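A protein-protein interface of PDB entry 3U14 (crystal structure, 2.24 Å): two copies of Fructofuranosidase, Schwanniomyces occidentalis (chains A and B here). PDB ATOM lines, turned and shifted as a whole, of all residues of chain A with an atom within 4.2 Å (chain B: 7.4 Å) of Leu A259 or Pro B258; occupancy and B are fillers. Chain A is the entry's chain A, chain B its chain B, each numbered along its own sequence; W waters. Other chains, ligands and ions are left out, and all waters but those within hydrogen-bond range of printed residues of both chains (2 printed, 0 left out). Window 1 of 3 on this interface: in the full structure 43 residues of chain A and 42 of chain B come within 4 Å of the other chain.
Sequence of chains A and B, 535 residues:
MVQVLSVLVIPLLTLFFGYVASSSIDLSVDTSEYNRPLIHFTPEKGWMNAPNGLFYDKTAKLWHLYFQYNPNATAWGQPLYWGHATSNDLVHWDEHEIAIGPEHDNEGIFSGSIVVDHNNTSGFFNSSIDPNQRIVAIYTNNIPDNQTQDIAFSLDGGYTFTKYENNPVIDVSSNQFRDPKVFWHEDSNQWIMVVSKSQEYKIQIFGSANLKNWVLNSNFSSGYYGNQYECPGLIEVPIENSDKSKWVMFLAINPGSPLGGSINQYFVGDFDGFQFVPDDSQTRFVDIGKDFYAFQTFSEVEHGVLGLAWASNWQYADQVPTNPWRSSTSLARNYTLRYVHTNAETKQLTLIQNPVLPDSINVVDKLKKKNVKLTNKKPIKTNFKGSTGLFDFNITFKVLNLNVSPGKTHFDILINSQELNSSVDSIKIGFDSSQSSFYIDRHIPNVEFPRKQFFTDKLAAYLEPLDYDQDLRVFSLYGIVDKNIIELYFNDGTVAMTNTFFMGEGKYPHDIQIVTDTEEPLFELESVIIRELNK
Of the 10 printed residues of chain A, 4 touch a printed residue of chain B.
Printed residues of chain A that touch a printed residue of chain B: Pro A258, Leu A259, Phe A285 and Thr A456.
Hydrophobic or aromatic side chains of chain A within 4 Å of the printed part of chain B: Leu A259 and Phe A285.
Among the printed residues, pairs that only touch across the chains: Leu A259 with Pro B258 (3.4 Å), Pro A258 with Leu B259 (3.5 Å), Phe A285 with Tyr B224 (3.6 Å) and Thr A456 with Lys B458 (3.8 Å).
Water W2 lies within hydrogen-bond range of the side-chain hydroxyl of Tyr B224 (2.8 Å) and the backbone NH of Phe A285 (3.1 Å).
Water W1 bridges the backbone NH (N) of Ala B460 (3.0 Å) and the backbone carbonyl oxygen (O) of Leu A259 (3.2 Å).
Ser A257 touches none of the printed residues of chain B.
Leu A259 touches just one residue of chain B: Pro B258.
No residue of chain B comes within 4 Å of Gly A260.
Printed residues of chain B within 4 Å of Phe A285: Tyr B224 (3.6 Å).
Of the printed residues of chain B, Thr A456 touches Lys B458.
Printed residues of chain A within 4 Å of Tyr B224: Phe A285 (3.6 Å).
Gly B226 touches none of the printed residues of chain A.
Pro B258 touches just one residue of chain A: Leu A259.
Printed residues of chain A within 4 Å of Leu B259: Pro A258 (3.5 Å).
Printed residues of chain A within 4 Å of Lys B458: Thr A456 (3.8 Å).
The nearest printed residue of chain A that does not touch Pro B258 is Phe A285 (4.2 Å).
The nearest printed residue of chain A that does not touch Lys B458 is Leu A259 (6.2 Å).
The backbone NH of Leu A259 lies within hydrogen-bond range of the side-chain hydroxyl of Ser A257.
NZ of Lys A290 sits close to O of Leu A259 (3.3 Å).
The side-chain amino group (NZ) of Lys A290 sits at hydrogen-bond distance from the side-chain hydroxyl (OG1) of Thr A456, 3.3 Å away.
OG of Ser B257 lies within hydrogen-bond range of N of Leu B259 (3.0 Å).
The side-chain amino group (NZ) of Lys B290 sits close to the backbone carbonyl oxygen (O) of Leu B259 (3.2 Å).
Pro A258 touches Leu B259, and with the chains exchanged Leu A259 touches Pro B258.
7 positions are printed for both chains.
Of the 4 pairs that touch across the chains among the printed residues, 2 have their exchanged pair printed and touching as well.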
ATOM      1  N   SER A 257       0.481  20.340 -32.907  1.00  0.00           N
ATOM      2  CA  SER A 257       0.994  20.667 -31.577  1.00  0.00           C
ATOM      3  C   SER A 257       2.273  21.497 -31.705  1.00  0.00           C
ATOM      4  O   SER A 257       3.096  21.210 -32.579  1.00  0.00           O
ATOM      5  CB  SER A 257       1.287  19.399 -30.788  1.00  0.00           C
ATOM      6  OG  SER A 257       2.150  19.690 -29.690  1.00  0.00           O
ATOM      7  N   PRO A 258       2.444  22.535 -30.845  1.00  0.00           N
ATOM      8  CA  PRO A 258       3.673  23.322 -30.872  1.00  0.00           C
ATOM      9  C   PRO A 258       4.883  22.471 -30.497  1.00  0.00           C
ATOM     10  O   PRO A 258       6.020  22.845 -30.798  1.00  0.00           O
ATOM     11  CB  PRO A 258       3.433  24.396 -29.808  1.00  0.00           C
ATOM     12  CG  PRO A 258       2.407  23.832 -28.919  1.00  0.00           C
ATOM     13  CD  PRO A 258       1.532  22.989 -29.782  1.00  0.00           C
ATOM     14  N   LEU A 259       4.639  21.327 -29.862  1.00  0.00           N
ATOM     15  CA  LEU A 259       5.718  20.382 -29.569  1.00  0.00           C
ATOM     16  C   LEU A 259       5.927  19.417 -30.739  1.00  0.00           C
ATOM     17  O   LEU A 259       6.842  18.610 -30.718  1.00  0.00           O
ATOM     18  CB  LEU A 259       5.434  19.624 -28.274  1.00  0.00           C
ATOM     19  CG  LEU A 259       5.820  20.308 -26.938  1.00  0.00           C
ATOM     20  CD1 LEU A 259       4.894  21.458 -26.571  1.00  0.00           C
ATOM     21  CD2 LEU A 259       5.857  19.298 -25.797  1.00  0.00           C
ATOM     22  N   GLY A 260       5.086  19.530 -31.764  1.00  0.00           N
ATOM     23  CA  GLY A 260       5.090  18.588 -32.879  1.00  0.00           C
ATOM     24  C   GLY A 260       4.076  17.470 -32.666  1.00  0.00           C
ATOM     25  O   GLY A 260       4.122  16.753 -31.667  1.00  0.00           O
ATOM     26  N   ILE A 263      -1.012  16.694 -29.046  1.00  0.00           N
ATOM     27  CA  ILE A 263      -0.970  17.135 -27.656  1.00  0.00           C
ATOM     28  C   ILE A 263      -2.403  17.342 -27.118  1.00  0.00           C
ATOM     29  O   ILE A 263      -3.330  17.553 -27.901  1.00  0.00           O
ATOM     30  CB  ILE A 263      -0.113  18.416 -27.506  1.00  0.00           C
ATOM     31  CG1 ILE A 263       0.432  18.542 -26.076  1.00  0.00           C
ATOM     32  CG2 ILE A 263      -0.891  19.683 -27.996  1.00  0.00           C
ATOM     33  CD1 ILE A 263       1.457  19.649 -25.880  1.00  0.00           C
ATOM     34  N   PHE A 285      -1.418  23.213 -21.643  1.00  0.00           N
ATOM     35  CA  PHE A 285      -1.437  21.795 -22.004  1.00  0.00           C
ATOM     36  C   PHE A 285      -1.523  20.892 -20.777  1.00  0.00           C
ATOM     37  O   PHE A 285      -1.008  21.226 -19.693  1.00  0.00           O
ATOM     38  CB  PHE A 285      -0.249  21.455 -22.892  1.00  0.00           C
ATOM     39  CG  PHE A 285      -0.204  22.269 -24.159  1.00  0.00           C
ATOM     40  CD1 PHE A 285       0.780  23.261 -24.347  1.00  0.00           C
ATOM     41  CD2 PHE A 285      -1.160  22.070 -25.152  1.00  0.00           C
ATOM     42  CE1 PHE A 285       0.814  24.028 -25.523  1.00  0.00           C
ATOM     43  CE2 PHE A 285      -1.151  22.826 -26.336  1.00  0.00           C
ATOM     44  CZ  PHE A 285      -0.162  23.810 -26.534  1.00  0.00           C
ATOM     45  N   ILE A 288       3.044  18.097 -20.974  1.00  0.00           N
ATOM     46  CA  ILE A 288       3.970  18.709 -21.934  1.00  0.00           C
ATOM     47  C   ILE A 288       5.109  17.803 -22.303  1.00  0.00           C
ATOM     48  O   ILE A 288       6.196  18.272 -22.637  1.00  0.00           O
ATOM     49  CB  ILE A 288       4.582  20.035 -21.438  1.00  0.00           C
ATOM     50  CG1 ILE A 288       5.044  19.902 -19.980  1.00  0.00           C
ATOM     51  CG2 ILE A 288       3.642  21.177 -21.720  1.00  0.00           C
ATOM     52  CD1 ILE A 288       6.071  20.951 -19.567  1.00  0.00           C
ATOM     53  N   GLY A 289       4.873  16.502 -22.221  1.00  0.00           N
ATOM     54  CA  GLY A 289       5.741  15.558 -22.894  1.00  0.00           C
ATOM     55  C   GLY A 289       5.198  15.345 -24.298  1.00  0.00           C
ATOM     56  O   GLY A 289       4.148  15.871 -24.692  1.00  0.00           O
ATOM     57  N   LYS A 290       5.898  14.531 -25.051  1.00  0.00           N
ATOM     58  CA  LYS A 290       5.581  14.363 -26.436  1.00  0.00           C
ATOM     59  C   LYS A 290       4.471  13.309 -26.630  1.00  0.00           C
ATOM     60  O   LYS A 290       3.863  13.261 -27.700  1.00  0.00           O
ATOM     61  CB  LYS A 290       6.881  13.958 -27.095  1.00  0.00           C
ATOM     62  CG  LYS A 290       7.021  14.266 -28.488  1.00  0.00           C
ATOM     63  CD  LYS A 290       7.621  15.529 -28.920  1.00  0.00           C
ATOM     64  CE  LYS A 290       6.830  15.905 -30.158  1.00  0.00           C
ATOM     65  NZ  LYS A 290       7.324  15.454 -31.472  1.00  0.00           N
ATOM     66  N   THR A 456      11.393  14.063 -30.814  1.00  0.00           N
ATOM     67  CA  THR A 456      12.133  15.043 -30.030  1.00  0.00           C
ATOM     68  C   THR A 456      12.809  14.384 -28.811  1.00  0.00           C
ATOM     69  O   THR A 456      12.178  13.639 -28.059  1.00  0.00           O
ATOM     70  CB  THR A 456      11.204  16.198 -29.581  1.00  0.00           C
ATOM     71  OG1 THR A 456      10.328  16.556 -30.663  1.00  0.00           O
ATOM     72  CG2 THR A 456      12.009  17.403 -29.157  1.00  0.00           C
ATOM     73  N   TYR B 224      -0.649  32.394 -24.476  1.00  0.00           N
ATOM     74  CA  TYR B 224       0.188  31.490 -23.691  1.00  0.00           C
ATOM     75  C   TYR B 224       0.895  32.309 -22.630  1.00  0.00           C
ATOM     76  O   TYR B 224       1.668  33.220 -22.958  1.00  0.00           O
ATOM     77  CB  TYR B 224       1.208  30.765 -24.577  1.00  0.00           C
ATOM     78  CG  TYR B 224       1.649  29.456 -23.979  1.00  0.00           C
ATOM     79  CD1 TYR B 224       0.996  28.271 -24.311  1.00  0.00           C
ATOM     80  CD2 TYR B 224       2.695  29.401 -23.055  1.00  0.00           C
ATOM     81  CE1 TYR B 224       1.378  27.069 -23.762  1.00  0.00           C
ATOM     82  CE2 TYR B 224       3.088  28.188 -22.501  1.00  0.00           C
ATOM     83  CZ  TYR B 224       2.420  27.026 -22.862  1.00  0.00           C
ATOM     84  OH  TYR B 224       2.786  25.817 -22.336  1.00  0.00           O
ATOM     85  N   GLY B 226       3.087  31.403 -19.806  1.00  0.00           N
ATOM     86  CA  GLY B 226       4.505  31.261 -19.473  1.00  0.00           C
ATOM     87  C   GLY B 226       4.790  31.841 -18.098  1.00  0.00           C
ATOM     88  O   GLY B 226       3.887  31.960 -17.263  1.00  0.00           O
ATOM     89  N   ILE B 253       6.991  36.041 -24.338  1.00  0.00           N
ATOM     90  CA  ILE B 253       7.018  35.426 -23.016  1.00  0.00           C
ATOM     91  C   ILE B 253       8.332  34.693 -22.778  1.00  0.00           C
ATOM     92  O   ILE B 253       8.880  34.105 -23.703  1.00  0.00           O
ATOM     93  CB  ILE B 253       5.824  34.498 -22.791  1.00  0.00           C
ATOM     94  CG1 ILE B 253       5.719  33.452 -23.914  1.00  0.00           C
ATOM     95  CG2 ILE B 253       4.524  35.303 -22.699  1.00  0.00           C
ATOM     96  CD1 ILE B 253       5.260  32.126 -23.412  1.00  0.00           C
ATOM     97  N   PRO B 255      10.635  33.067 -18.944  1.00  0.00           N
ATOM     98  CA  PRO B 255      10.679  31.681 -19.468  1.00  0.00           C
ATOM     99  C   PRO B 255       9.273  31.083 -19.623  1.00  0.00           C
ATOM    100  O   PRO B 255       8.269  31.818 -19.499  1.00  0.00           O
ATOM    101  CB  PRO B 255      11.495  30.926 -18.412  1.00  0.00           C
ATOM    102  CG  PRO B 255      11.423  31.758 -17.183  1.00  0.00           C
ATOM    103  CD  PRO B 255      11.314  33.189 -17.643  1.00  0.00           C
ATOM    104  N   GLY B 256       9.198  29.779 -19.911  1.00  0.00           N
ATOM    105  CA  GLY B 256       7.920  29.075 -19.951  1.00  0.00           C
ATOM    106  C   GLY B 256       7.255  28.911 -21.312  1.00  0.00           C
ATOM    107  O   GLY B 256       6.072  28.542 -21.390  1.00  0.00           O
ATOM    108  N   SER B 257       7.994  29.193 -22.383  1.00  0.00           N
ATOM    109  CA  SER B 257       7.572  28.832 -23.737  1.00  0.00           C
ATOM    110  C   SER B 257       7.335  27.318 -23.796  1.00  0.00           C
ATOM    111  O   SER B 257       8.083  26.545 -23.180  1.00  0.00           O
ATOM    112  CB  SER B 257       8.654  29.216 -24.755  1.00  0.00           C
ATOM    113  OG  SER B 257       8.571  28.432 -25.950  1.00  0.00           O
ATOM    114  N   PRO B 258       6.293  26.882 -24.526  1.00  0.00           N
ATOM    115  CA  PRO B 258       6.053  25.452 -24.646  1.00  0.00           C
ATOM    116  C   PRO B 258       7.176  24.750 -25.411  1.00  0.00           C
ATOM    117  O   PRO B 258       7.289  23.524 -25.327  1.00  0.00           O
ATOM    118  CB  PRO B 258       4.752  25.391 -25.443  1.00  0.00           C
ATOM    119  CG  PRO B 258       4.743  26.634 -26.215  1.00  0.00           C
ATOM    120  CD  PRO B 258       5.295  27.656 -25.280  1.00  0.00           C
ATOM    121  N   LEU B 259       7.986  25.521 -26.140  1.00  0.00           N
ATOM    122  CA  LEU B 259       9.179  25.003 -26.784  1.00  0.00           C
ATOM    123  C   LEU B 259      10.367  25.056 -25.837  1.00  0.00           C
ATOM    124  O   LEU B 259      11.446  24.593 -26.173  1.00  0.00           O
ATOM    125  CB  LEU B 259       9.479  25.755 -28.079  1.00  0.00           C
ATOM    126  CG  LEU B 259       8.707  25.344 -29.346  1.00  0.00           C
ATOM    127  CD1 LEU B 259       7.210  25.717 -29.259  1.00  0.00           C
ATOM    128  CD2 LEU B 259       9.333  25.968 -30.576  1.00  0.00           C
ATOM    129  N   GLY B 260      10.164  25.595 -24.642  1.00  0.00           N
ATOM    130  CA  GLY B 260      11.274  25.845 -23.709  1.00  0.00           C
ATOM    131  C   GLY B 260      11.909  27.227 -23.856  1.00  0.00           C
ATOM    132  O   GLY B 260      12.374  27.619 -24.932  1.00  0.00           O
ATOM    133  N   GLY B 261      11.910  27.976 -22.767  1.00  0.00           N
ATOM    134  CA  GLY B 261      12.556  29.277 -22.730  1.00  0.00           C
ATOM    135  C   GLY B 261      11.703  30.413 -23.272  1.00  0.00           C
ATOM    136  O   GLY B 261      10.598  30.668 -22.781  1.00  0.00           O
ATOM    137  N   SER B 262      12.225  31.087 -24.290  1.00  0.00           N
ATOM    138  CA  SER B 262      11.643  32.310 -24.787  1.00  0.00           C
ATOM    139  C   SER B 262      11.006  32.111 -26.157  1.00  0.00           C
ATOM    140  O   SER B 262      11.539  31.379 -27.006  1.00  0.00           O
ATOM    141  CB  SER B 262      12.722  33.393 -24.853  1.00  0.00           C
ATOM    142  OG  SER B 262      13.895  32.915 -25.514  1.00  0.00           O
ATOM    143  N   ILE B 263       9.860  32.760 -26.366  1.00  0.00           N
ATOM    144  CA  ILE B 263       9.133  32.712 -27.643  1.00  0.00           C
ATOM    145  C   ILE B 263       8.230  33.955 -27.780  1.00  0.00           C
ATOM    146  O   ILE B 263       7.858  34.578 -26.769  1.00  0.00           O
ATOM    147  CB  ILE B 263       8.287  31.401 -27.753  1.00  0.00           C
ATOM    148  CG1 ILE B 263       8.030  31.027 -29.206  1.00  0.00           C
ATOM    149  CG2 ILE B 263       6.982  31.510 -26.935  1.00  0.00           C
ATOM    150  CD1 ILE B 263       7.469  29.625 -29.395  1.00  0.00           C
ATOM    151  N   THR B 283      -4.280  30.945 -29.632  1.00  0.00           N
ATOM    152  CA  THR B 283      -2.881  31.226 -29.389  1.00  0.00           C
ATOM    153  C   THR B 283      -2.106  30.847 -30.643  1.00  0.00           C
ATOM    154  O   THR B 283      -2.334  29.775 -31.224  1.00  0.00           O
ATOM    155  CB  THR B 283      -2.371  30.418 -28.176  1.00  0.00           C
ATOM    156  OG1 THR B 283      -2.859  31.015 -26.970  1.00  0.00           O
ATOM    157  CG2 THR B 283      -0.864  30.393 -28.121  1.00  0.00           C
ATOM    158  N   PHE B 285       2.101  31.504 -32.421  1.00  0.00           N
ATOM    159  CA  PHE B 285       3.450  32.021 -32.246  1.00  0.00           C
ATOM    160  C   PHE B 285       3.960  32.685 -33.524  1.00  0.00           C
ATOM    161  O   PHE B 285       3.607  32.281 -34.634  1.00  0.00           O
ATOM    162  CB  PHE B 285       4.371  30.921 -31.753  1.00  0.00           C
ATOM    163  CG  PHE B 285       3.990  30.383 -30.394  1.00  0.00           C
ATOM    164  CD1 PHE B 285       3.544  29.079 -30.254  1.00  0.00           C
ATOM    165  CD2 PHE B 285       4.066  31.192 -29.258  1.00  0.00           C
ATOM    166  CE1 PHE B 285       3.192  28.565 -28.993  1.00  0.00           C
ATOM    167  CE2 PHE B 285       3.699  30.705 -27.990  1.00  0.00           C
ATOM    168  CZ  PHE B 285       3.268  29.378 -27.853  1.00  0.00           C
ATOM    169  N   LYS B 290      13.491  28.003 -31.967  1.00  0.00           N
ATOM    170  CA  LYS B 290      13.850  28.292 -30.585  1.00  0.00           C
ATOM    171  C   LYS B 290      14.394  29.687 -30.362  1.00  0.00           C
ATOM    172  O   LYS B 290      14.411  30.162 -29.230  1.00  0.00           O
ATOM    173  CB  LYS B 290      14.841  27.269 -30.047  1.00  0.00           C
ATOM    174  CG  LYS B 290      14.115  26.036 -29.610  1.00  0.00           C
ATOM    175  CD  LYS B 290      14.539  25.380 -28.381  1.00  0.00           C
ATOM    176  CE  LYS B 290      13.828  25.868 -27.166  1.00  0.00           C
ATOM    177  NZ  LYS B 290      14.517  25.293 -25.981  1.00  0.00           N
ATOM    178  N   LYS B 458      15.757  18.953 -32.498  1.00  0.00           N
ATOM    179  CA  LYS B 458      14.757  18.538 -33.479  1.00  0.00           C
ATOM    180  C   LYS B 458      13.458  19.361 -33.337  1.00  0.00           C
ATOM    181  O   LYS B 458      12.794  19.324 -32.298  1.00  0.00           O
ATOM    182  CB  LYS B 458      14.479  17.037 -33.348  1.00  0.00           C
ATOM    183  CG  LYS B 458      15.663  16.124 -33.750  1.00  0.00           C
ATOM    184  CD  LYS B 458      15.296  14.621 -33.614  1.00  0.00           C
ATOM    185  CE  LYS B 458      16.412  13.717 -34.122  1.00  0.00           C
ATOM    186  NZ  LYS B 458      16.028  12.274 -34.067  1.00  0.00           N
ATOM    187  N   LEU B 459      13.110  20.100 -34.381  1.00  0.00           N
ATOM    188  CA  LEU B 459      11.936  20.961 -34.367  1.00  0.00           C
ATOM    189  C   LEU B 459      11.178  20.798 -35.664  1.00  0.00           C
ATOM    190  O   LEU B 459      11.793  20.662 -36.722  1.00  0.00           O
ATOM    191  CB  LEU B 459      12.351  22.412 -34.212  1.00  0.00           C
ATOM    192  CG  LEU B 459      13.145  22.774 -32.954  1.00  0.00           C
ATOM    193  CD1 LEU B 459      13.989  23.983 -33.232  1.00  0.00           C
ATOM    194  CD2 LEU B 459      12.220  22.998 -31.740  1.00  0.00           C
ATOM    195  N   ALA B 460       9.851  20.819 -35.603  1.00  0.00           N
ATOM    196  CA  ALA B 460       9.044  20.544 -36.806  1.00  0.00           C
ATOM    197  C   ALA B 460       8.009  21.630 -37.022  1.00  0.00           C
ATOM    198  O   ALA B 460       7.770  22.463 -36.133  1.00  0.00           O
ATOM    199  CB  ALA B 460       8.362  19.172 -36.709  1.00  0.00           C
HETATM  200  O   HOH W   1       8.419  20.001 -33.115  1.00  0.00           O
HETATM  201  O   HOH W   2       1.161  24.448 -20.569  1.00  0.00           O
